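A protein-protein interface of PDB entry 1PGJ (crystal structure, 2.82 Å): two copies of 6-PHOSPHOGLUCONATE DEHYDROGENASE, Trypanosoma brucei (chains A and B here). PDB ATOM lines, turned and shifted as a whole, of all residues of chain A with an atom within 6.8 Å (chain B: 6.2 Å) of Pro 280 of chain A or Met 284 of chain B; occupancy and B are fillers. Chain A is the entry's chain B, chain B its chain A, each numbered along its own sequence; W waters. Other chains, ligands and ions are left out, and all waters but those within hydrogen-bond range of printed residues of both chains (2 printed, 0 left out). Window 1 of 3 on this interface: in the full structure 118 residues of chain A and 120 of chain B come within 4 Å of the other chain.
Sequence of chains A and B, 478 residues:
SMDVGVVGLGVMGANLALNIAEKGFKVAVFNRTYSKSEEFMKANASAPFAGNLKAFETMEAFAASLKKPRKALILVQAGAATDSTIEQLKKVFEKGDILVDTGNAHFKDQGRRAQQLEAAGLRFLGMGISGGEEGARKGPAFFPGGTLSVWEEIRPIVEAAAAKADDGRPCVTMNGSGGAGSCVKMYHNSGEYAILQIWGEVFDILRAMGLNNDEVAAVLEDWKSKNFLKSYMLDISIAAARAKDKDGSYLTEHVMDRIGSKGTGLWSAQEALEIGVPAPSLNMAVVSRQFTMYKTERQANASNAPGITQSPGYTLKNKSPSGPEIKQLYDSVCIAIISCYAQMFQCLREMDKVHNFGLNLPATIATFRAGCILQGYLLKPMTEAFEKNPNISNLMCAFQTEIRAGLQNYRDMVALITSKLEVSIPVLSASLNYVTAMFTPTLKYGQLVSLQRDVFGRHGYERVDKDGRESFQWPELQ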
ATOM      1  N   VAL A 277      -1.771  -1.177  -5.710  1.00  0.00           N
ATOM      2  CA  VAL A 277      -2.843  -2.116  -5.386  1.00  0.00           C
ATOM      3  C   VAL A 277      -2.375  -3.107  -4.356  1.00  0.00           C
ATOM      4  O   VAL A 277      -1.308  -3.712  -4.501  1.00  0.00           O
ATOM      5  CB  VAL A 277      -3.319  -2.962  -6.595  1.00  0.00           C
ATOM      6  CG1 VAL A 277      -4.578  -3.731  -6.216  1.00  0.00           C
ATOM      7  CG2 VAL A 277      -3.614  -2.106  -7.779  1.00  0.00           C
ATOM      8  N   PRO A 278      -3.198  -3.315  -3.316  1.00  0.00           N
ATOM      9  CA  PRO A 278      -2.923  -4.249  -2.212  1.00  0.00           C
ATOM     10  C   PRO A 278      -2.978  -5.719  -2.620  1.00  0.00           C
ATOM     11  O   PRO A 278      -4.028  -6.248  -2.972  1.00  0.00           O
ATOM     12  CB  PRO A 278      -4.002  -3.895  -1.186  1.00  0.00           C
ATOM     13  CG  PRO A 278      -5.093  -3.291  -2.005  1.00  0.00           C
ATOM     14  CD  PRO A 278      -4.368  -2.474  -3.019  1.00  0.00           C
ATOM     15  N   ALA A 279      -1.832  -6.385  -2.548  1.00  0.00           N
ATOM     16  CA  ALA A 279      -1.737  -7.793  -2.896  1.00  0.00           C
ATOM     17  C   ALA A 279      -0.799  -8.444  -1.897  1.00  0.00           C
ATOM     18  O   ALA A 279       0.310  -8.886  -2.242  1.00  0.00           O
ATOM     19  CB  ALA A 279      -1.185  -7.943  -4.293  1.00  0.00           C
ATOM     20  N   PRO A 280      -1.241  -8.538  -0.631  1.00  0.00           N
ATOM     21  CA  PRO A 280      -0.379  -9.151   0.379  1.00  0.00           C
ATOM     22  C   PRO A 280       0.038 -10.611   0.088  1.00  0.00           C
ATOM     23  O   PRO A 280       1.198 -10.964   0.273  1.00  0.00           O
ATOM     24  CB  PRO A 280      -1.201  -8.970   1.652  1.00  0.00           C
ATOM     25  CG  PRO A 280      -2.556  -9.061   1.191  1.00  0.00           C
ATOM     26  CD  PRO A 280      -2.571  -8.262  -0.090  1.00  0.00           C
ATOM     27  N   SER A 281      -0.867 -11.432  -0.430  1.00  0.00           N
ATOM     28  CA  SER A 281      -0.534 -12.820  -0.728  1.00  0.00           C
ATOM     29  C   SER A 281       0.468 -12.940  -1.896  1.00  0.00           C
ATOM     30  O   SER A 281       1.348 -13.830  -1.908  1.00  0.00           O
ATOM     31  CB  SER A 281      -1.805 -13.612  -1.047  1.00  0.00           C
ATOM     32  OG  SER A 281      -2.770 -13.422  -0.048  1.00  0.00           O
ATOM     33  N   LEU A 282       0.344 -12.056  -2.885  1.00  0.00           N
ATOM     34  CA  LEU A 282       1.250 -12.118  -4.036  1.00  0.00           C
ATOM     35  C   LEU A 282       2.652 -11.691  -3.617  1.00  0.00           C
ATOM     36  O   LEU A 282       3.667 -12.260  -4.042  1.00  0.00           O
ATOM     37  CB  LEU A 282       0.742 -11.240  -5.169  1.00  0.00           C
ATOM     38  CG  LEU A 282      -0.704 -11.414  -5.608  1.00  0.00           C
ATOM     39  CD1 LEU A 282      -0.825 -10.929  -7.041  1.00  0.00           C
ATOM     40  CD2 LEU A 282      -1.100 -12.892  -5.468  1.00  0.00           C
ATOM     41  N   ASN A 283       2.684 -10.726  -2.711  1.00  0.00           N
ATOM     42  CA  ASN A 283       3.916 -10.194  -2.164  1.00  0.00           C
ATOM     43  C   ASN A 283       4.646 -11.171  -1.245  1.00  0.00           C
ATOM     44  O   ASN A 283       5.847 -11.348  -1.381  1.00  0.00           O
ATOM     45  CB  ASN A 283       3.584  -8.893  -1.436  1.00  0.00           C
ATOM     46  CG  ASN A 283       3.873  -7.662  -2.284  1.00  0.00           C
ATOM     47  OD1 ASN A 283       4.949  -7.108  -2.214  1.00  0.00           O
ATOM     48  ND2 ASN A 283       2.886  -7.226  -3.102  1.00  0.00           N
ATOM     49  N   MET A 284       3.931 -11.805  -0.315  1.00  0.00           N
ATOM     50  CA  MET A 284       4.544 -12.785   0.605  1.00  0.00           C
ATOM     51  C   MET A 284       4.909 -14.098  -0.071  1.00  0.00           C
ATOM     52  O   MET A 284       5.712 -14.861   0.444  1.00  0.00           O
ATOM     53  CB  MET A 284       3.630 -13.112   1.773  1.00  0.00           C
ATOM     54  CG  MET A 284       3.405 -11.951   2.693  1.00  0.00           C
ATOM     55  SD  MET A 284       4.911 -11.471   3.552  1.00  0.00           S
ATOM     56  CE  MET A 284       5.497 -13.037   4.160  1.00  0.00           C
ATOM     57  N   ALA A 285       4.284 -14.379  -1.205  1.00  0.00           N
ATOM     58  CA  ALA A 285       4.590 -15.591  -1.933  1.00  0.00           C
ATOM     59  C   ALA A 285       6.073 -15.514  -2.345  1.00  0.00           C
ATOM     60  O   ALA A 285       6.843 -16.460  -2.140  1.00  0.00           O
ATOM     61  CB  ALA A 285       3.677 -15.706  -3.138  1.00  0.00           C
ATOM     62  N   GLN A 343      -6.993 -11.006  -5.436  1.00  0.00           N
ATOM     63  CA  GLN A 343      -5.864 -10.079  -5.509  1.00  0.00           C
ATOM     64  C   GLN A 343      -5.332 -10.028  -6.946  1.00  0.00           C
ATOM     65  O   GLN A 343      -5.193  -8.961  -7.550  1.00  0.00           O
ATOM     66  CB  GLN A 343      -4.750 -10.551  -4.564  1.00  0.00           C
ATOM     67  CG  GLN A 343      -4.982 -10.209  -3.085  1.00  0.00           C
ATOM     68  CD  GLN A 343      -4.134 -11.043  -2.081  1.00  0.00           C
ATOM     69  OE1 GLN A 343      -2.891 -10.998  -2.053  1.00  0.00           O
ATOM     70  NE2 GLN A 343      -4.826 -11.783  -1.235  1.00  0.00           N
ATOM     71  N   PRO A 426       3.522 -17.882   6.054  1.00  0.00           N
ATOM     72  CA  PRO A 426       3.499 -16.556   5.412  1.00  0.00           C
ATOM     73  C   PRO A 426       2.218 -16.269   4.608  1.00  0.00           C
ATOM     74  O   PRO A 426       1.474 -15.336   4.905  1.00  0.00           O
ATOM     75  CB  PRO A 426       4.712 -16.594   4.465  1.00  0.00           C
ATOM     76  CG  PRO A 426       5.629 -17.611   5.066  1.00  0.00           C
ATOM     77  CD  PRO A 426       4.711 -18.667   5.647  1.00  0.00           C
ATOM     78  N   VAL A 427       1.933 -17.078   3.599  1.00  0.00           N
ATOM     79  CA  VAL A 427       0.782 -16.800   2.763  1.00  0.00           C
ATOM     80  C   VAL A 427      -0.571 -17.161   3.355  1.00  0.00           C
ATOM     81  O   VAL A 427      -1.545 -16.438   3.123  1.00  0.00           O
ATOM     82  CB  VAL A 427       0.981 -17.316   1.329  1.00  0.00           C
ATOM     83  CG1 VAL A 427      -0.229 -16.944   0.443  1.00  0.00           C
ATOM     84  CG2 VAL A 427       2.237 -16.730   0.767  1.00  0.00           C
ATOM     85  N   SER A 429      -1.335 -16.726   6.222  1.00  0.00           N
ATOM     86  CA  SER A 429      -1.510 -15.592   7.107  1.00  0.00           C
ATOM     87  C   SER A 429      -1.878 -14.307   6.398  1.00  0.00           C
ATOM     88  O   SER A 429      -2.841 -13.653   6.774  1.00  0.00           O
ATOM     89  CB  SER A 429      -0.253 -15.342   7.908  1.00  0.00           C
ATOM     90  OG  SER A 429      -0.562 -14.391   8.900  1.00  0.00           O
ATOM     91  N   ALA A 430      -1.078 -13.914   5.415  1.00  0.00           N
ATOM     92  CA  ALA A 430      -1.340 -12.686   4.674  1.00  0.00           C
ATOM     93  C   ALA A 430      -2.705 -12.697   4.038  1.00  0.00           C
ATOM     94  O   ALA A 430      -3.426 -11.699   4.073  1.00  0.00           O
ATOM     95  CB  ALA A 430      -0.319 -12.481   3.621  1.00  0.00           C
ATOM     96  N   SER A 431      -3.096 -13.838   3.503  1.00  0.00           N
ATOM     97  CA  SER A 431      -4.393 -13.935   2.859  1.00  0.00           C
ATOM     98  C   SER A 431      -5.568 -13.667   3.809  1.00  0.00           C
ATOM     99  O   SER A 431      -6.570 -13.055   3.411  1.00  0.00           O
ATOM    100  CB  SER A 431      -4.529 -15.283   2.179  1.00  0.00           C
ATOM    101  OG  SER A 431      -3.359 -15.554   1.434  1.00  0.00           O
ATOM    102  N   ASN A 433      -5.467 -11.675   6.309  1.00  0.00           N
ATOM    103  CA  ASN A 433      -5.472 -10.246   6.573  1.00  0.00           C
ATOM    104  C   ASN A 433      -6.077  -9.511   5.392  1.00  0.00           C
ATOM    105  O   ASN A 433      -6.768  -8.514   5.574  1.00  0.00           O
ATOM    106  CB  ASN A 433      -4.073  -9.748   6.901  1.00  0.00           C
ATOM    107  CG  ASN A 433      -3.652 -10.097   8.325  1.00  0.00           C
ATOM    108  OD1 ASN A 433      -4.419  -9.947   9.280  1.00  0.00           O
ATOM    109  ND2 ASN A 433      -2.423 -10.537   8.475  1.00  0.00           N
ATOM    110  N   TYR A 434      -5.871 -10.053   4.190  1.00  0.00           N
ATOM    111  CA  TYR A 434      -6.422  -9.446   2.992  1.00  0.00           C
ATOM    112  C   TYR A 434      -7.937  -9.454   3.123  1.00  0.00           C
ATOM    113  O   TYR A 434      -8.600  -8.430   2.904  1.00  0.00           O
ATOM    114  CB  TYR A 434      -6.014 -10.217   1.724  1.00  0.00           C
ATOM    115  CG  TYR A 434      -6.547  -9.580   0.433  1.00  0.00           C
ATOM    116  CD1 TYR A 434      -6.094  -8.335   0.000  1.00  0.00           C
ATOM    117  CD2 TYR A 434      -7.533 -10.206  -0.316  1.00  0.00           C
ATOM    118  CE1 TYR A 434      -6.621  -7.737  -1.126  1.00  0.00           C
ATOM    119  CE2 TYR A 434      -8.053  -9.612  -1.437  1.00  0.00           C
ATOM    120  CZ  TYR A 434      -7.603  -8.379  -1.837  1.00  0.00           C
ATOM    121  OH  TYR A 434      -8.194  -7.788  -2.931  1.00  0.00           O
ATOM    122  N   VAL A 435      -8.486 -10.600   3.506  1.00  0.00           N
ATOM    123  CA  VAL A 435      -9.937 -10.677   3.653  1.00  0.00           C
ATOM    124  C   VAL A 435     -10.517  -9.742   4.720  1.00  0.00           C
ATOM    125  O   VAL A 435     -11.441  -8.997   4.437  1.00  0.00           O
ATOM    126  CB  VAL A 435     -10.417 -12.106   3.955  1.00  0.00           C
ATOM    127  CG1 VAL A 435     -11.941 -12.148   3.922  1.00  0.00           C
ATOM    128  CG2 VAL A 435      -9.806 -13.091   2.971  1.00  0.00           C
ATOM    129  N   GLN B 197       3.369   1.557  11.757  1.00  0.00           N
ATOM    130  CA  GLN B 197       2.248   0.649  11.551  1.00  0.00           C
ATOM    131  C   GLN B 197       2.073  -0.249  12.788  1.00  0.00           C
ATOM    132  O   GLN B 197       0.950  -0.587  13.166  1.00  0.00           O
ATOM    133  CB  GLN B 197       2.476  -0.199  10.299  1.00  0.00           C
ATOM    134  CG  GLN B 197       1.417  -1.266  10.055  1.00  0.00           C
ATOM    135  CD  GLN B 197       0.016  -0.695   9.912  1.00  0.00           C
ATOM    136  OE1 GLN B 197      -0.139   0.498   9.666  1.00  0.00           O
ATOM    137  NE2 GLN B 197      -1.019  -1.544  10.088  1.00  0.00           N
ATOM    138  N   ALA B 279      12.233  -9.527   3.698  1.00  0.00           N
ATOM    139  CA  ALA B 279      11.870  -8.450   4.575  1.00  0.00           C
ATOM    140  C   ALA B 279      10.348  -8.323   4.581  1.00  0.00           C
ATOM    141  O   ALA B 279       9.779  -7.320   4.089  1.00  0.00           O
ATOM    142  CB  ALA B 279      12.517  -7.183   4.072  1.00  0.00           C
ATOM    143  N   PRO B 280       9.656  -9.305   5.187  1.00  0.00           N
ATOM    144  CA  PRO B 280       8.189  -9.281   5.243  1.00  0.00           C
ATOM    145  C   PRO B 280       7.602  -8.031   5.914  1.00  0.00           C
ATOM    146  O   PRO B 280       6.683  -7.385   5.379  1.00  0.00           O
ATOM    147  CB  PRO B 280       7.859 -10.541   6.036  1.00  0.00           C
ATOM    148  CG  PRO B 280       8.970 -10.669   6.936  1.00  0.00           C
ATOM    149  CD  PRO B 280      10.169 -10.392   6.028  1.00  0.00           C
ATOM    150  N   SER B 281       8.158  -7.643   7.051  1.00  0.00           N
ATOM    151  CA  SER B 281       7.624  -6.483   7.745  1.00  0.00           C
ATOM    152  C   SER B 281       7.734  -5.207   6.921  1.00  0.00           C
ATOM    153  O   SER B 281       6.859  -4.357   6.966  1.00  0.00           O
ATOM    154  CB  SER B 281       8.328  -6.310   9.088  1.00  0.00           C
ATOM    155  OG  SER B 281       8.335  -7.532   9.776  1.00  0.00           O
ATOM    156  N   LEU B 282       8.829  -5.072   6.185  1.00  0.00           N
ATOM    157  CA  LEU B 282       9.043  -3.890   5.378  1.00  0.00           C
ATOM    158  C   LEU B 282       8.034  -3.814   4.255  1.00  0.00           C
ATOM    159  O   LEU B 282       7.579  -2.730   3.908  1.00  0.00           O
ATOM    160  CB  LEU B 282      10.457  -3.865   4.832  1.00  0.00           C
ATOM    161  CG  LEU B 282      11.540  -3.876   5.927  1.00  0.00           C
ATOM    162  CD1 LEU B 282      12.914  -3.446   5.340  1.00  0.00           C
ATOM    163  CD2 LEU B 282      11.106  -2.966   7.098  1.00  0.00           C
ATOM    164  N   ASN B 283       7.630  -4.958   3.726  1.00  0.00           N
ATOM    165  CA  ASN B 283       6.667  -4.949   2.645  1.00  0.00           C
ATOM    166  C   ASN B 283       5.294  -4.697   3.107  1.00  0.00           C
ATOM    167  O   ASN B 283       4.584  -3.946   2.495  1.00  0.00           O
ATOM    168  CB  ASN B 283       6.605  -6.299   1.976  1.00  0.00           C
ATOM    169  CG  ASN B 283       7.689  -6.488   1.015  1.00  0.00           C
ATOM    170  OD1 ASN B 283       7.527  -6.230  -0.170  1.00  0.00           O
ATOM    171  ND2 ASN B 283       8.858  -6.916   1.522  1.00  0.00           N
ATOM    172  N   MET B 284       4.873  -5.469   4.096  1.00  0.00           N
ATOM    173  CA  MET B 284       3.544  -5.345   4.615  1.00  0.00           C
ATOM    174  C   MET B 284       3.296  -3.992   5.211  1.00  0.00           C
ATOM    175  O   MET B 284       2.148  -3.619   5.434  1.00  0.00           O
ATOM    176  CB  MET B 284       3.249  -6.434   5.619  1.00  0.00           C
ATOM    177  CG  MET B 284       3.274  -7.804   4.973  1.00  0.00           C
ATOM    178  SD  MET B 284       1.797  -8.210   3.990  1.00  0.00           S
ATOM    179  CE  MET B 284       0.726  -8.376   5.256  1.00  0.00           C
ATOM    180  N   ALA B 285       4.354  -3.241   5.478  1.00  0.00           N
ATOM    181  CA  ALA B 285       4.156  -1.901   6.003  1.00  0.00           C
ATOM    182  C   ALA B 285       3.579  -1.074   4.850  1.00  0.00           C
ATOM    183  O   ALA B 285       2.642  -0.332   5.032  1.00  0.00           O
ATOM    184  CB  ALA B 285       5.462  -1.321   6.489  1.00  0.00           C
ATOM    185  N   VAL B 286       4.110  -1.247   3.646  1.00  0.00           N
ATOM    186  CA  VAL B 286       3.604  -0.536   2.494  1.00  0.00           C
ATOM    187  C   VAL B 286       2.229  -1.063   2.137  1.00  0.00           C
ATOM    188  O   VAL B 286       1.288  -0.268   1.938  1.00  0.00           O
ATOM    189  CB  VAL B 286       4.558  -0.643   1.322  1.00  0.00           C
ATOM    190  CG1 VAL B 286       3.852  -0.434   0.007  1.00  0.00           C
ATOM    191  CG2 VAL B 286       5.613   0.392   1.481  1.00  0.00           C
ATOM    192  N   VAL B 287       2.073  -2.387   2.139  1.00  0.00           N
ATOM    193  CA  VAL B 287       0.779  -2.991   1.804  1.00  0.00           C
ATOM    194  C   VAL B 287      -0.318  -2.483   2.743  1.00  0.00           C
ATOM    195  O   VAL B 287      -1.418  -2.150   2.296  1.00  0.00           O
ATOM    196  CB  VAL B 287       0.816  -4.547   1.835  1.00  0.00           C
ATOM    197  CG1 VAL B 287      -0.512  -5.097   1.363  1.00  0.00           C
ATOM    198  CG2 VAL B 287       1.937  -5.089   0.956  1.00  0.00           C
ATOM    199  N   SER B 288       0.008  -2.369   4.028  1.00  0.00           N
ATOM    200  CA  SER B 288      -0.933  -1.879   5.022  1.00  0.00           C
ATOM    201  C   SER B 288      -1.452  -0.494   4.622  1.00  0.00           C
ATOM    202  O   SER B 288      -2.621  -0.186   4.829  1.00  0.00           O
ATOM    203  CB  SER B 288      -0.278  -1.809   6.401  1.00  0.00           C
ATOM    204  OG  SER B 288       0.532  -0.649   6.555  1.00  0.00           O
ATOM    205  N   ARG B 289      -0.587   0.345   4.058  1.00  0.00           N
ATOM    206  CA  ARG B 289      -1.033   1.682   3.622  1.00  0.00           C
ATOM    207  C   ARG B 289      -1.906   1.537   2.395  1.00  0.00           C
ATOM    208  O   ARG B 289      -2.933   2.215   2.264  1.00  0.00           O
ATOM    209  CB  ARG B 289       0.132   2.618   3.282  1.00  0.00           C
ATOM    210  CG  ARG B 289       0.949   3.015   4.480  1.00  0.00           C
ATOM    211  CD  ARG B 289       1.876   4.156   4.142  1.00  0.00           C
ATOM    212  NE  ARG B 289       2.839   4.380   5.218  1.00  0.00           N
ATOM    213  CZ  ARG B 289       3.450   5.535   5.467  1.00  0.00           C
ATOM    214  NH1 ARG B 289       3.197   6.606   4.710  1.00  0.00           N
ATOM    215  NH2 ARG B 289       4.331   5.611   6.464  1.00  0.00           N
ATOM    216  N   PHE B 291      -3.795  -0.792   1.790  1.00  0.00           N
ATOM    217  CA  PHE B 291      -5.122  -1.155   2.303  1.00  0.00           C
ATOM    218  C   PHE B 291      -5.965   0.093   2.550  1.00  0.00           C
ATOM    219  O   PHE B 291      -7.067   0.188   2.070  1.00  0.00           O
ATOM    220  CB  PHE B 291      -5.036  -1.892   3.635  1.00  0.00           C
ATOM    221  CG  PHE B 291      -4.720  -3.342   3.512  1.00  0.00           C
ATOM    222  CD1 PHE B 291      -4.914  -4.010   2.315  1.00  0.00           C
ATOM    223  CD2 PHE B 291      -4.190  -4.045   4.601  1.00  0.00           C
ATOM    224  CE1 PHE B 291      -4.584  -5.361   2.183  1.00  0.00           C
ATOM    225  CE2 PHE B 291      -3.860  -5.387   4.483  1.00  0.00           C
ATOM    226  CZ  PHE B 291      -4.059  -6.051   3.258  1.00  0.00           C
ATOM    227  N   ILE B 425      -4.101  -7.204  11.323  1.00  0.00           N
ATOM    228  CA  ILE B 425      -2.778  -6.935  11.891  1.00  0.00           C
ATOM    229  C   ILE B 425      -1.678  -7.389  10.894  1.00  0.00           C
ATOM    230  O   ILE B 425      -0.895  -8.306  11.161  1.00  0.00           O
ATOM    231  CB  ILE B 425      -2.623  -7.581  13.324  1.00  0.00           C
ATOM    232  CG1 ILE B 425      -2.889  -9.084  13.283  1.00  0.00           C
ATOM    233  CG2 ILE B 425      -3.559  -6.934  14.320  1.00  0.00           C
ATOM    234  CD1 ILE B 425      -2.474  -9.791  14.544  1.00  0.00           C
ATOM    235  N   PRO B 426      -1.552  -6.676   9.762  1.00  0.00           N
ATOM    236  CA  PRO B 426      -0.577  -6.979   8.712  1.00  0.00           C
ATOM    237  C   PRO B 426       0.837  -7.137   9.205  1.00  0.00           C
ATOM    238  O   PRO B 426       1.434  -8.186   9.067  1.00  0.00           O
ATOM    239  CB  PRO B 426      -0.653  -5.749   7.804  1.00  0.00           C
ATOM    240  CG  PRO B 426      -1.985  -5.249   8.014  1.00  0.00           C
ATOM    241  CD  PRO B 426      -2.202  -5.394   9.480  1.00  0.00           C
ATOM    242  N   VAL B 427       1.350  -6.070   9.796  1.00  0.00           N
ATOM    243  CA  VAL B 427       2.707  -6.024  10.271  1.00  0.00           C
ATOM    244  C   VAL B 427       3.021  -6.872  11.520  1.00  0.00           C
ATOM    245  O   VAL B 427       4.030  -7.597  11.556  1.00  0.00           O
ATOM    246  CB  VAL B 427       3.168  -4.542  10.353  1.00  0.00           C
ATOM    247  CG1 VAL B 427       4.502  -4.430  11.009  1.00  0.00           C
ATOM    248  CG2 VAL B 427       3.305  -3.994   8.965  1.00  0.00           C
ATOM    249  N   ALA B 430       3.186 -10.413   9.977  1.00  0.00           N
ATOM    250  CA  ALA B 430       4.349 -10.670   9.132  1.00  0.00           C
ATOM    251  C   ALA B 430       5.648 -10.789   9.954  1.00  0.00           C
ATOM    252  O   ALA B 430       6.523 -11.644   9.682  1.00  0.00           O
ATOM    253  CB  ALA B 430       4.486  -9.586   8.104  1.00  0.00           C
HETATM  254  O   HOH W   1       5.882  -8.662   0.136  1.00  0.00           O
HETATM  255  O   HOH W   2       0.065 -10.563   7.117  1.00  0.00           O
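N of Ile 425 of chain B lies within hydrogen-bond range of OD1 of Asn 433 of chain A, at 3.4 Å.
The side-chain amide oxygen of Asn 283 of chain A sits close to the side-chain amide oxygen of Asn 283 of chain B, 3.4 Å away.
The side-chain amide nitrogen of Asn 283 of chain B lies within hydrogen-bond range of the backbone carbonyl oxygen of Ala 279 of chain B (2.8 Å).
O of Ala 279 of chain A is in hydrogen-bond range of ND2 of Asn 283 of chain A.
CD1 of Phe 291 of chain B touches CB of Pro 278 of chain A (3.6 Å).
Pro 280 of chain A touches Met 284 of chain B.
Pro 280 of chain A touches Val 287 of chain B (CB to CG1, 3.9 Å).
Phe 291 of chain B touches Pro 280 of chain A (CZ to CG, 3.9 Å).
CB of Pro 280 of chain B touches CE of Met 284 of chain A, at 3.9 Å.
Phe 291 of chain B touches Tyr 434 of chain A (CE1 to CD1, 3.99 Å).
Of the printed residues of chain B, Pro 278 of chain A touches Phe 291 (3.6 Å).
Printed residues of chain B within 4 Å of Pro 280 of chain A: Met 284, Val 287 and Phe 291.
Of the printed residues of chain B, Asn 283 of chain A touches Asn 283 (3.4 Å).
Of the printed residues of chain A, Pro 280 of chain B touches Met 284.
Of the printed residues of chain A, Asn 283 of chain B touches Asn 283.
Printed residues of chain A within 4 Å of Met 284 of chain B: Pro 280.
Printed residues of chain A within 4 Å of Phe 291 of chain B: Pro 278, Pro 280 and Tyr 434.
The nearest printed residue of chain B that does not touch Pro 280 of chain A is Pro 426 of chain B (7.0 Å).
The nearest residue of chain A that does not touch Met 284 of chain B is Met 284 of chain A (4.3 Å).
The nearest printed residue of chain B that does not touch Asn 433 of chain A is Pro 426 of chain B (4.02 Å).
Of the 17 printed residues of chain B, 6 touch a printed residue of chain A.
Printed residues of chain B that touch a printed residue of chain A: Pro 280, Asn 283, Met 284, Val 287, Phe 291 and Ile 425.
Along chain B the printed residues that touch a printed residue of chain A span positions 280 to 425.
Among the printed residues, no Asp or Glu carboxylate lies within 4 Å of a Lys or Arg side-chain nitrogen of the other chain.
Pro 280 of chain A touches Met 284 of chain B, and with the chains exchanged Met 284 of chain A touches Pro 280 of chain B.
Asn 283 of chain A touches its own counterpart, Asn 283 of chain B.
Water W2 bridges ND2 of Asn 433 of chain A (2.8 Å) and O of Pro 426 of chain B (3.4 Å).
Water W1 lies within hydrogen-bond range of OD1 of Asn 283 of chain B (3.0 Å) and OD1 of Asn 283 of chain A (3.0 Å).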
